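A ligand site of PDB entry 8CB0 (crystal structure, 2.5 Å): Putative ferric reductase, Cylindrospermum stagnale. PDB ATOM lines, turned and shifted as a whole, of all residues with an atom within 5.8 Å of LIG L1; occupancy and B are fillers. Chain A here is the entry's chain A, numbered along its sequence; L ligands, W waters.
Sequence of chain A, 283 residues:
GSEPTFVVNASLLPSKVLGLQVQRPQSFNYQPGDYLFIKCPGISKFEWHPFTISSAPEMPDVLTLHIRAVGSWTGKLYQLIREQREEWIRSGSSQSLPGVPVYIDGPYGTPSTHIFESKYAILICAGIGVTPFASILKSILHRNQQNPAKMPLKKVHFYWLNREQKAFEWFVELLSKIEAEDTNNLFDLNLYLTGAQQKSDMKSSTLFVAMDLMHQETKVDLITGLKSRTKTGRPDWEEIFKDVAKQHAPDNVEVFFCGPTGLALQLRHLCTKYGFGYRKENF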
ATOM      1  N   TYR A  35      -1.362  30.352 -37.188  1.00  0.00           N
ATOM      2  CA  TYR A  35      -1.378  30.284 -35.706  1.00  0.00           C
ATOM      3  C   TYR A  35      -2.342  31.321 -35.171  1.00  0.00           C
ATOM      4  O   TYR A  35      -2.853  32.169 -35.913  1.00  0.00           O
ATOM      5  CB  TYR A  35       0.020  30.434 -35.146  1.00  0.00           C
ATOM      6  CG  TYR A  35       0.722  31.759 -35.331  1.00  0.00           C
ATOM      7  CD1 TYR A  35       1.442  32.039 -36.474  1.00  0.00           C
ATOM      8  CD2 TYR A  35       0.769  32.684 -34.284  1.00  0.00           C
ATOM      9  CE1 TYR A  35       2.111  33.247 -36.613  1.00  0.00           C
ATOM     10  CE2 TYR A  35       1.467  33.876 -34.391  1.00  0.00           C
ATOM     11  CZ  TYR A  35       2.123  34.161 -35.577  1.00  0.00           C
ATOM     12  OH  TYR A  35       2.829  35.322 -35.659  1.00  0.00           O
ATOM     13  N   GLU A  47      -2.277  37.277 -19.945  1.00  0.00           N
ATOM     14  CA  GLU A  47      -1.204  36.680 -20.787  1.00  0.00           C
ATOM     15  C   GLU A  47      -1.792  36.021 -22.039  1.00  0.00           C
ATOM     16  O   GLU A  47      -2.784  35.279 -21.925  1.00  0.00           O
ATOM     17  CB  GLU A  47      -0.423  35.627 -20.028  1.00  0.00           C
ATOM     18  CG  GLU A  47       0.847  36.153 -19.444  1.00  0.00           C
ATOM     19  CD  GLU A  47       1.872  35.132 -18.991  1.00  0.00           C
ATOM     20  OE1 GLU A  47       1.708  33.929 -19.292  1.00  0.00           O
ATOM     21  OE2 GLU A  47       2.830  35.549 -18.312  1.00  0.00           O
ATOM     22  N   HIS A  49      -0.597  33.550 -25.326  1.00  0.00           N
ATOM     23  CA  HIS A  49       0.413  32.638 -25.904  1.00  0.00           C
ATOM     24  C   HIS A  49      -0.020  32.203 -27.283  1.00  0.00           C
ATOM     25  O   HIS A  49      -1.194  32.031 -27.576  1.00  0.00           O
ATOM     26  CB  HIS A  49       0.672  31.428 -25.001  1.00  0.00           C
ATOM     27  CG  HIS A  49       1.302  31.808 -23.717  1.00  0.00           C
ATOM     28  ND1 HIS A  49       2.613  31.546 -23.457  1.00  0.00           N
ATOM     29  CD2 HIS A  49       0.797  32.452 -22.645  1.00  0.00           C
ATOM     30  CE1 HIS A  49       2.899  31.985 -22.247  1.00  0.00           C
ATOM     31  NE2 HIS A  49       1.785  32.541 -21.716  1.00  0.00           N
ATOM     32  N   PRO A  50       0.973  32.037 -28.195  1.00  0.00           N
ATOM     33  CA  PRO A  50       0.697  31.600 -29.550  1.00  0.00           C
ATOM     34  C   PRO A  50       0.792  30.080 -29.757  1.00  0.00           C
ATOM     35  O   PRO A  50       1.729  29.447 -29.360  1.00  0.00           O
ATOM     36  CB  PRO A  50       1.780  32.357 -30.330  1.00  0.00           C
ATOM     37  CG  PRO A  50       2.972  32.400 -29.404  1.00  0.00           C
ATOM     38  CD  PRO A  50       2.371  32.460 -28.021  1.00  0.00           C
ATOM     39  N   PHE A  51      -0.167  29.562 -30.492  1.00  0.00           N
ATOM     40  CA  PHE A  51      -0.194  28.132 -30.827  1.00  0.00           C
ATOM     41  C   PHE A  51      -0.636  28.004 -32.267  1.00  0.00           C
ATOM     42  O   PHE A  51      -1.523  28.779 -32.738  1.00  0.00           O
ATOM     43  CB  PHE A  51      -1.084  27.378 -29.837  1.00  0.00           C
ATOM     44  CG  PHE A  51      -0.538  27.400 -28.427  1.00  0.00           C
ATOM     45  CD1 PHE A  51       0.555  26.632 -28.082  1.00  0.00           C
ATOM     46  CD2 PHE A  51      -1.094  28.217 -27.475  1.00  0.00           C
ATOM     47  CE1 PHE A  51       1.097  26.693 -26.801  1.00  0.00           C
ATOM     48  CE2 PHE A  51      -0.565  28.298 -26.201  1.00  0.00           C
ATOM     49  CZ  PHE A  51       0.539  27.543 -25.866  1.00  0.00           C
ATOM     50  N   THR A  52       0.020  27.073 -32.948  1.00  0.00           N
ATOM     51  CA  THR A  52      -0.314  26.652 -34.326  1.00  0.00           C
ATOM     52  C   THR A  52      -1.694  26.019 -34.263  1.00  0.00           C
ATOM     53  O   THR A  52      -1.988  25.264 -33.292  1.00  0.00           O
ATOM     54  CB  THR A  52       0.783  25.728 -34.865  1.00  0.00           C
ATOM     55  OG1 THR A  52       1.988  26.471 -35.046  1.00  0.00           O
ATOM     56  CG2 THR A  52       0.445  25.134 -36.197  1.00  0.00           C
ATOM     57  N   ILE A  53      -2.528  26.339 -35.238  1.00  0.00           N
ATOM     58  CA  ILE A  53      -3.814  25.632 -35.430  1.00  0.00           C
ATOM     59  C   ILE A  53      -3.502  24.296 -36.126  1.00  0.00           C
ATOM     60  O   ILE A  53      -3.138  24.277 -37.333  1.00  0.00           O
ATOM     61  CB  ILE A  53      -4.745  26.533 -36.253  1.00  0.00           C
ATOM     62  CG1 ILE A  53      -4.959  27.877 -35.579  1.00  0.00           C
ATOM     63  CG2 ILE A  53      -6.053  25.812 -36.487  1.00  0.00           C
ATOM     64  CD1 ILE A  53      -5.903  28.818 -36.325  1.00  0.00           C
ATOM     65  N   HIS A  66      -2.398  21.583 -30.440  1.00  0.00           N
ATOM     66  CA  HIS A  66      -1.569  20.607 -29.705  1.00  0.00           C
ATOM     67  C   HIS A  66      -0.558  21.396 -28.894  1.00  0.00           C
ATOM     68  O   HIS A  66       0.424  21.889 -29.442  1.00  0.00           O
ATOM     69  CB  HIS A  66      -0.956  19.578 -30.660  1.00  0.00           C
ATOM     70  CG  HIS A  66      -1.973  18.626 -31.164  1.00  0.00           C
ATOM     71  ND1 HIS A  66      -2.942  18.992 -32.062  1.00  0.00           N
ATOM     72  CD2 HIS A  66      -2.166  17.309 -30.900  1.00  0.00           C
ATOM     73  CE1 HIS A  66      -3.704  17.952 -32.311  1.00  0.00           C
ATOM     74  NE2 HIS A  66      -3.265  16.918 -31.595  1.00  0.00           N
ATOM     75  N   ILE A  67      -0.799  21.512 -27.606  1.00  0.00           N
ATOM     76  CA  ILE A  67       0.012  22.388 -26.716  1.00  0.00           C
ATOM     77  C   ILE A  67       0.851  21.492 -25.827  1.00  0.00           C
ATOM     78  O   ILE A  67       0.296  20.679 -25.168  1.00  0.00           O
ATOM     79  CB  ILE A  67      -0.942  23.273 -25.899  1.00  0.00           C
ATOM     80  CG1 ILE A  67      -1.719  24.204 -26.814  1.00  0.00           C
ATOM     81  CG2 ILE A  67      -0.148  24.052 -24.880  1.00  0.00           C
ATOM     82  CD1 ILE A  67      -2.721  25.116 -26.092  1.00  0.00           C
ATOM     83  N   ARG A  68       2.152  21.591 -25.887  1.00  0.00           N
ATOM     84  CA  ARG A  68       3.038  20.790 -24.999  1.00  0.00           C
ATOM     85  C   ARG A  68       3.400  21.578 -23.720  1.00  0.00           C
ATOM     86  O   ARG A  68       3.869  22.727 -23.853  1.00  0.00           O
ATOM     87  CB  ARG A  68       4.325  20.435 -25.728  1.00  0.00           C
ATOM     88  CG  ARG A  68       5.212  19.463 -24.985  1.00  0.00           C
ATOM     89  CD  ARG A  68       6.368  19.054 -25.846  1.00  0.00           C
ATOM     90  NE  ARG A  68       7.013  17.935 -25.201  1.00  0.00           N
ATOM     91  CZ  ARG A  68       8.231  17.955 -24.688  1.00  0.00           C
ATOM     92  NH1 ARG A  68       8.981  19.031 -24.775  1.00  0.00           N
ATOM     93  NH2 ARG A  68       8.700  16.875 -24.098  1.00  0.00           N
ATOM     94  N   ALA A  69       3.252  20.944 -22.552  1.00  0.00           N
ATOM     95  CA  ALA A  69       3.557  21.509 -21.215  1.00  0.00           C
ATOM     96  C   ALA A  69       5.059  21.667 -21.082  1.00  0.00           C
ATOM     97  O   ALA A  69       5.711  20.680 -20.864  1.00  0.00           O
ATOM     98  CB  ALA A  69       3.057  20.593 -20.142  1.00  0.00           C
ATOM     99  N   VAL A  70       5.583  22.872 -21.240  1.00  0.00           N
ATOM    100  CA  VAL A  70       7.051  23.111 -21.234  1.00  0.00           C
ATOM    101  C   VAL A  70       7.460  24.083 -20.134  1.00  0.00           C
ATOM    102  O   VAL A  70       8.645  24.252 -19.972  1.00  0.00           O
ATOM    103  CB  VAL A  70       7.484  23.676 -22.583  1.00  0.00           C
ATOM    104  CG1 VAL A  70       7.392  22.611 -23.646  1.00  0.00           C
ATOM    105  CG2 VAL A  70       6.635  24.902 -22.913  1.00  0.00           C
ATOM    106  N   GLY A  71       6.508  24.781 -19.521  1.00  0.00           N
ATOM    107  CA  GLY A  71       6.764  25.793 -18.492  1.00  0.00           C
ATOM    108  C   GLY A  71       5.497  26.211 -17.777  1.00  0.00           C
ATOM    109  O   GLY A  71       4.536  25.432 -17.641  1.00  0.00           O
ATOM    110  N   SER A  72       5.451  27.481 -17.435  1.00  0.00           N
ATOM    111  CA  SER A  72       4.511  27.999 -16.438  1.00  0.00           C
ATOM    112  C   SER A  72       3.081  27.924 -17.012  1.00  0.00           C
ATOM    113  O   SER A  72       2.260  27.210 -16.465  1.00  0.00           O
ATOM    114  CB  SER A  72       4.979  29.397 -16.030  1.00  0.00           C
ATOM    115  OG  SER A  72       3.967  30.041 -15.277  1.00  0.00           O
ATOM    116  N   TRP A  73       2.768  28.676 -18.043  1.00  0.00           N
ATOM    117  CA  TRP A  73       1.370  28.785 -18.536  1.00  0.00           C
ATOM    118  C   TRP A  73       0.909  27.436 -19.108  1.00  0.00           C
ATOM    119  O   TRP A  73      -0.176  27.013 -18.734  1.00  0.00           O
ATOM    120  CB  TRP A  73       1.282  29.897 -19.582  1.00  0.00           C
ATOM    121  CG  TRP A  73      -0.071  30.287 -20.034  1.00  0.00           C
ATOM    122  CD1 TRP A  73      -0.750  31.378 -19.615  1.00  0.00           C
ATOM    123  CD2 TRP A  73      -0.867  29.680 -21.045  1.00  0.00           C
ATOM    124  NE1 TRP A  73      -1.935  31.480 -20.285  1.00  0.00           N
ATOM    125  CE2 TRP A  73      -2.032  30.436 -21.150  1.00  0.00           C
ATOM    126  CE3 TRP A  73      -0.718  28.567 -21.876  1.00  0.00           C
ATOM    127  CZ2 TRP A  73      -3.049  30.114 -22.040  1.00  0.00           C
ATOM    128  CZ3 TRP A  73      -1.717  28.241 -22.753  1.00  0.00           C
ATOM    129  CH2 TRP A  73      -2.870  29.000 -22.842  1.00  0.00           C
ATOM    130  N   THR A  74       1.713  26.777 -19.944  1.00  0.00           N
ATOM    131  CA  THR A  74       1.307  25.480 -20.565  1.00  0.00           C
ATOM    132  C   THR A  74       1.167  24.438 -19.454  1.00  0.00           C
ATOM    133  O   THR A  74       0.228  23.643 -19.531  1.00  0.00           O
ATOM    134  CB  THR A  74       2.242  25.034 -21.709  1.00  0.00           C
ATOM    135  OG1 THR A  74       3.596  24.862 -21.284  1.00  0.00           O
ATOM    136  CG2 THR A  74       2.234  26.021 -22.852  1.00  0.00           C
ATOM    137  N   GLY A  75       2.043  24.455 -18.445  1.00  0.00           N
ATOM    138  CA  GLY A  75       1.956  23.536 -17.294  1.00  0.00           C
ATOM    139  C   GLY A  75       0.642  23.721 -16.541  1.00  0.00           C
ATOM    140  O   GLY A  75       0.013  22.724 -16.144  1.00  0.00           O
ATOM    141  N   THR A 110       2.010  32.431 -41.766  1.00  0.00           N
ATOM    142  CA  THR A 110       3.408  31.957 -41.868  1.00  0.00           C
ATOM    143  C   THR A 110       3.644  31.658 -43.344  1.00  0.00           C
ATOM    144  O   THR A 110       2.706  31.416 -44.106  1.00  0.00           O
ATOM    145  CB  THR A 110       3.720  30.707 -41.021  1.00  0.00           C
ATOM    146  OG1 THR A 110       3.308  29.524 -41.696  1.00  0.00           O
ATOM    147  CG2 THR A 110       3.073  30.763 -39.654  1.00  0.00           C
ATOM    148  N   ILE A 128       7.056  18.979 -31.253  1.00  0.00           N
ATOM    149  CA  ILE A 128       5.738  19.659 -31.383  1.00  0.00           C
ATOM    150  C   ILE A 128       5.787  20.666 -32.559  1.00  0.00           C
ATOM    151  O   ILE A 128       4.719  21.145 -32.983  1.00  0.00           O
ATOM    152  CB  ILE A 128       5.343  20.333 -30.035  1.00  0.00           C
ATOM    153  CG1 ILE A 128       3.829  20.587 -29.935  1.00  0.00           C
ATOM    154  CG2 ILE A 128       6.111  21.601 -29.795  1.00  0.00           C
ATOM    155  CD1 ILE A 128       3.043  19.334 -30.214  1.00  0.00           C
ATOM    156  N   THR A 131       3.281  20.651 -35.683  1.00  0.00           N
ATOM    157  CA  THR A 131       1.851  21.044 -35.681  1.00  0.00           C
ATOM    158  C   THR A 131       1.439  21.763 -36.958  1.00  0.00           C
ATOM    159  O   THR A 131       0.354  21.494 -37.460  1.00  0.00           O
ATOM    160  CB  THR A 131       1.498  21.816 -34.417  1.00  0.00           C
ATOM    161  OG1 THR A 131       2.425  22.871 -34.267  1.00  0.00           O
ATOM    162  CG2 THR A 131       1.537  20.914 -33.187  1.00  0.00           C
ATOM    163  N   PRO A 132       2.202  22.717 -37.506  1.00  0.00           N
ATOM    164  CA  PRO A 132       1.752  23.392 -38.723  1.00  0.00           C
ATOM    165  C   PRO A 132       1.746  22.427 -39.917  1.00  0.00           C
ATOM    166  O   PRO A 132       0.930  22.616 -40.807  1.00  0.00           O
ATOM    167  CB  PRO A 132       2.788  24.524 -38.926  1.00  0.00           C
ATOM    168  CG  PRO A 132       4.008  24.089 -38.146  1.00  0.00           C
ATOM    169  CD  PRO A 132       3.451  23.297 -36.991  1.00  0.00           C
HETATM  170  P1  LIG L   1       7.803  29.269 -20.203  1.00  0.00           P
HETATM  171  O1  LIG L   1       7.949  30.516 -20.981  1.00  0.00           O
HETATM  172  O2  LIG L   1       7.495  29.269 -18.746  1.00  0.00           O
HETATM  173  O3  LIG L   1       9.110  28.376 -20.500  1.00  0.00           O
HETATM  174  C1  LIG L   1       9.492  28.189 -21.889  1.00  0.00           C
HETATM  175  C2  LIG L   1      10.883  27.611 -22.017  1.00  0.00           C
HETATM  176  O4  LIG L   1      11.854  28.627 -21.655  1.00  0.00           O
HETATM  177  C3  LIG L   1      11.210  26.406 -21.152  1.00  0.00           C
HETATM  178  O5  LIG L   1      12.140  25.563 -21.822  1.00  0.00           O
HETATM  179  C4  LIG L   1      11.839  27.052 -19.915  1.00  0.00           C
HETATM  180  O6  LIG L   1      12.703  26.192 -19.225  1.00  0.00           O
HETATM  181  C5  LIG L   1      12.615  28.202 -20.544  1.00  0.00           C
HETATM  182  N1  LIG L   1      12.818  29.338 -19.624  1.00  0.00           N
HETATM  183  C6  LIG L   1      11.848  30.060 -18.940  1.00  0.00           C
HETATM  184  N2  LIG L   1      12.365  30.990 -18.172  1.00  0.00           N
HETATM  185  C7  LIG L   1      13.739  30.874 -18.358  1.00  0.00           C
HETATM  186  C8  LIG L   1      14.838  31.579 -17.820  1.00  0.00           C
HETATM  187  N3  LIG L   1      14.689  32.563 -16.942  1.00  0.00           N
HETATM  188  N4  LIG L   1      16.083  31.212 -18.217  1.00  0.00           N
HETATM  189  C9  LIG L   1      16.209  30.198 -19.099  1.00  0.00           C
HETATM  190  N5  LIG L   1      15.251  29.460 -19.670  1.00  0.00           N
HETATM  191  C10 LIG L   1      14.034  29.853 -19.248  1.00  0.00           C
HETATM  192  N6  LIG L   1       3.948  25.332 -28.604  1.00  0.00           N
HETATM  193  C11 LIG L   1       3.204  24.209 -28.650  1.00  0.00           C
HETATM  194  O7  LIG L   1       3.223  23.423 -27.700  1.00  0.00           O
HETATM  195  N7  LIG L   1       2.376  23.900 -29.716  1.00  0.00           N
HETATM  196  C12 LIG L   1       2.361  24.681 -30.843  1.00  0.00           C
HETATM  197  O8  LIG L   1       1.661  24.375 -31.791  1.00  0.00           O
HETATM  198  C13 LIG L   1       3.072  25.880 -30.812  1.00  0.00           C
HETATM  199  N8  LIG L   1       2.965  26.670 -31.848  1.00  0.00           N
HETATM  200  C14 LIG L   1       3.648  27.862 -31.758  1.00  0.00           C
HETATM  201  C15 LIG L   1       3.542  28.736 -32.860  1.00  0.00           C
HETATM  202  C16 LIG L   1       4.212  29.929 -32.898  1.00  0.00           C
HETATM  203  C17 LIG L   1       4.058  30.821 -34.106  1.00  0.00           C
HETATM  204  C18 LIG L   1       4.991  30.305 -31.796  1.00  0.00           C
HETATM  205  C19 LIG L   1       5.743  31.614 -31.813  1.00  0.00           C
HETATM  206  C20 LIG L   1       5.118  29.467 -30.702  1.00  0.00           C
HETATM  207  C21 LIG L   1       4.445  28.233 -30.643  1.00  0.00           C
HETATM  208  N9  LIG L   1       4.534  27.350 -29.551  1.00  0.00           N
HETATM  209  C22 LIG L   1       3.851  26.162 -29.617  1.00  0.00           C
HETATM  210  C23 LIG L   1       5.281  27.703 -28.297  1.00  0.00           C
HETATM  211  C24 LIG L   1       4.409  28.406 -27.182  1.00  0.00           C
HETATM  212  O9  LIG L   1       3.692  29.465 -27.827  1.00  0.00           O
HETATM  213  C25 LIG L   1       4.612  28.505 -25.465  1.00  0.00           C
HETATM  214  O10 LIG L   1       4.323  29.934 -24.976  1.00  0.00           O
HETATM  215  C26 LIG L   1       5.648  28.107 -25.007  1.00  0.00           C
HETATM  216  O11 LIG L   1       5.638  26.940 -25.862  1.00  0.00           O
HETATM  217  C27 LIG L   1       4.833  28.152 -23.716  1.00  0.00           C
HETATM  218  O12 LIG L   1       5.152  29.186 -22.648  1.00  0.00           O
HETATM  219  P2  LIG L   1       5.060  28.793 -21.066  1.00  0.00           P
HETATM  220  O13 LIG L   1       4.694  29.869 -20.122  1.00  0.00           O
HETATM  221  O14 LIG L   1       4.286  27.547 -20.756  1.00  0.00           O
HETATM  222  O15 LIG L   1       6.573  28.407 -20.793  1.00  0.00           O
HETATM  223  O1  LG2 L   2       7.684  34.619 -36.771  1.00  0.00           O
HETATM  224  C1  LG2 L   2       8.747  35.370 -37.287  1.00  0.00           C
HETATM  225  C2  LG2 L   2       9.349  34.413 -38.335  1.00  0.00           C
HETATM  226  O2  LG2 L   2       8.484  33.287 -38.356  1.00  0.00           O
HETATM  227  C3  LG2 L   2       8.015  33.237 -36.998  1.00  0.00           C
HETATM  228  C4  LG2 L   2       9.156  32.799 -36.011  1.00  0.00           C
HETATM  229  C5  LG2 L   2       8.589  31.870 -34.911  1.00  0.00           C
HETATM  230  C6  LG2 L   2       6.714  32.410 -36.970  1.00  0.00           C
HETATM  231  C7  LG2 L   2       7.104  30.950 -36.865  1.00  0.00           C
HETATM  232  N1  LG2 L   2       7.752  30.749 -35.502  1.00  0.00           N
HETATM  233  C8  LG2 L   2       7.435  29.491 -34.685  1.00  0.00           C
HETATM  234  C9  LG2 L   2       8.059  29.397 -33.461  1.00  0.00           C
HETATM  235  C10 LG2 L   2       7.814  28.295 -32.638  1.00  0.00           C
HETATM  236  C11 LG2 L   2       6.921  27.229 -32.924  1.00  0.00           C
HETATM  237  C12 LG2 L   2       8.497  28.301 -31.437  1.00  0.00           C
HETATM  238  C13 LG2 L   2       9.348  29.407 -31.203  1.00  0.00           C
HETATM  239  C14 LG2 L   2      10.022  29.357 -29.986  1.00  0.00           C
HETATM  240  C15 LG2 L   2       9.880  28.308 -29.022  1.00  0.00           C
HETATM  241  C16 LG2 L   2       9.017  27.227 -29.276  1.00  0.00           C
HETATM  242  C17 LG2 L   2       8.317  27.217 -30.501  1.00  0.00           C
HETATM  243  C18 LG2 L   2       7.448  26.117 -30.786  1.00  0.00           C
HETATM  244  O3  LG2 L   2       7.322  25.202 -29.945  1.00  0.00           O
HETATM  245  C19 LG2 L   2       6.741  26.119 -32.021  1.00  0.00           C
HETATM  246  C20 LG2 L   2       5.847  25.056 -32.344  1.00  0.00           C
HETATM  247  C21 LG2 L   2       5.134  25.088 -33.567  1.00  0.00           C
HETATM  248  C22 LG2 L   2       5.314  26.183 -34.467  1.00  0.00           C
HETATM  249  C23 LG2 L   2       6.236  27.261 -34.155  1.00  0.00           C
HETATM  250  N2  LG2 L   2       6.501  28.398 -35.049  1.00  0.00           N
HETATM  251  O   HOH W   1       7.695  31.819 -16.993  1.00  0.00           O
HETATM  252  O   HOH W   2       4.360  24.777 -25.486  1.00  0.00           O
HETATM  253  O   HOH W   3       9.091  28.040 -17.198  1.00  0.00           O
HETATM  254  O   HOH W   4       7.225  24.291 -27.380  1.00  0.00           O
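OG1 of Thr 131 lies within hydrogen-bond range of O of Ile 128 (3.1 Å).
The side-chain hydroxyl of Thr 74 lies within hydrogen-bond range of the backbone NH of Val 70 (2.8 Å).
OG1 of Thr 74 lies within hydrogen-bond range of N of Gly 71, at 3.4 Å.
NE2 of His 49 sits at hydrogen-bond distance from OE1 of Glu 47, at 2.8 Å.
OG1 of Thr 74 lies within hydrogen-bond range of O of Arg 68 (3.4 Å).
Water W2 bridges O11 of LIG L1 and O of Arg 68.
Water W4 lies within hydrogen-bond range of O3 of LG2 L2 (2.7 Å) and O11 of LIG L1 (3.4 Å).
ND1 of His 49 sits at hydrogen-bond distance from O10 of LIG L1, at 2.8 Å.
OG1 of Thr 74 sits at hydrogen-bond distance from O14 of LIG L1, at 2.8 Å.
The side-chain hydroxyl (OG1) of Thr 52 lies within hydrogen-bond range of a nitrogen (N8) of LIG L1.
The backbone NH (N) of Trp 73 is in hydrogen-bond range of an oxygen (O13) of LIG L1 (3.1 Å).
A nitrogen (N7) of LIG L1 lies within hydrogen-bond range of the backbone carbonyl oxygen (O) of His 66, 2.8 Å away.
The side-chain hydroxyl of Thr 131 is in hydrogen-bond range of an oxygen (O8) of LIG L1, 3.0 Å away.
N of Thr 74 sits at hydrogen-bond distance from O14 of LIG L1 (2.8 Å).
The backbone NH (N) of Arg 68 lies within hydrogen-bond range of an oxygen (O7) of LIG L1, at 2.8 Å.
O of Pro 50 sits at hydrogen-bond distance from O9 of LIG L1, 2.5 Å away.
N of Thr 52 sits at hydrogen-bond distance from N8 of LIG L1, at 3.2 Å.
N of Ser 72 is in hydrogen-bond range of O2 of LIG L1, at 3.0 Å.
Merely in contact with LIG L1: Tyr 35, Phe 51, Ile 67, Val 70, Gly 71 and Ile 128.
Hydrophobic or aromatic side chains within 4 Å of LIG L1: Tyr 35, His 49, Pro 50, Phe 51, Val 70, Trp 73 and Ile 128.
15 residues have an atom within 4 Å of LIG L1: Tyr 35, His 49, Pro 50, Phe 51, Thr 52, His 66, Ile 67, Arg 68, Val 70, Gly 71, Ser 72, Trp 73, Thr 74, Ile 128 and Thr 131.
The nearest printed residue that does not touch LIG L1 is Gly 75 (4.5 Å).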
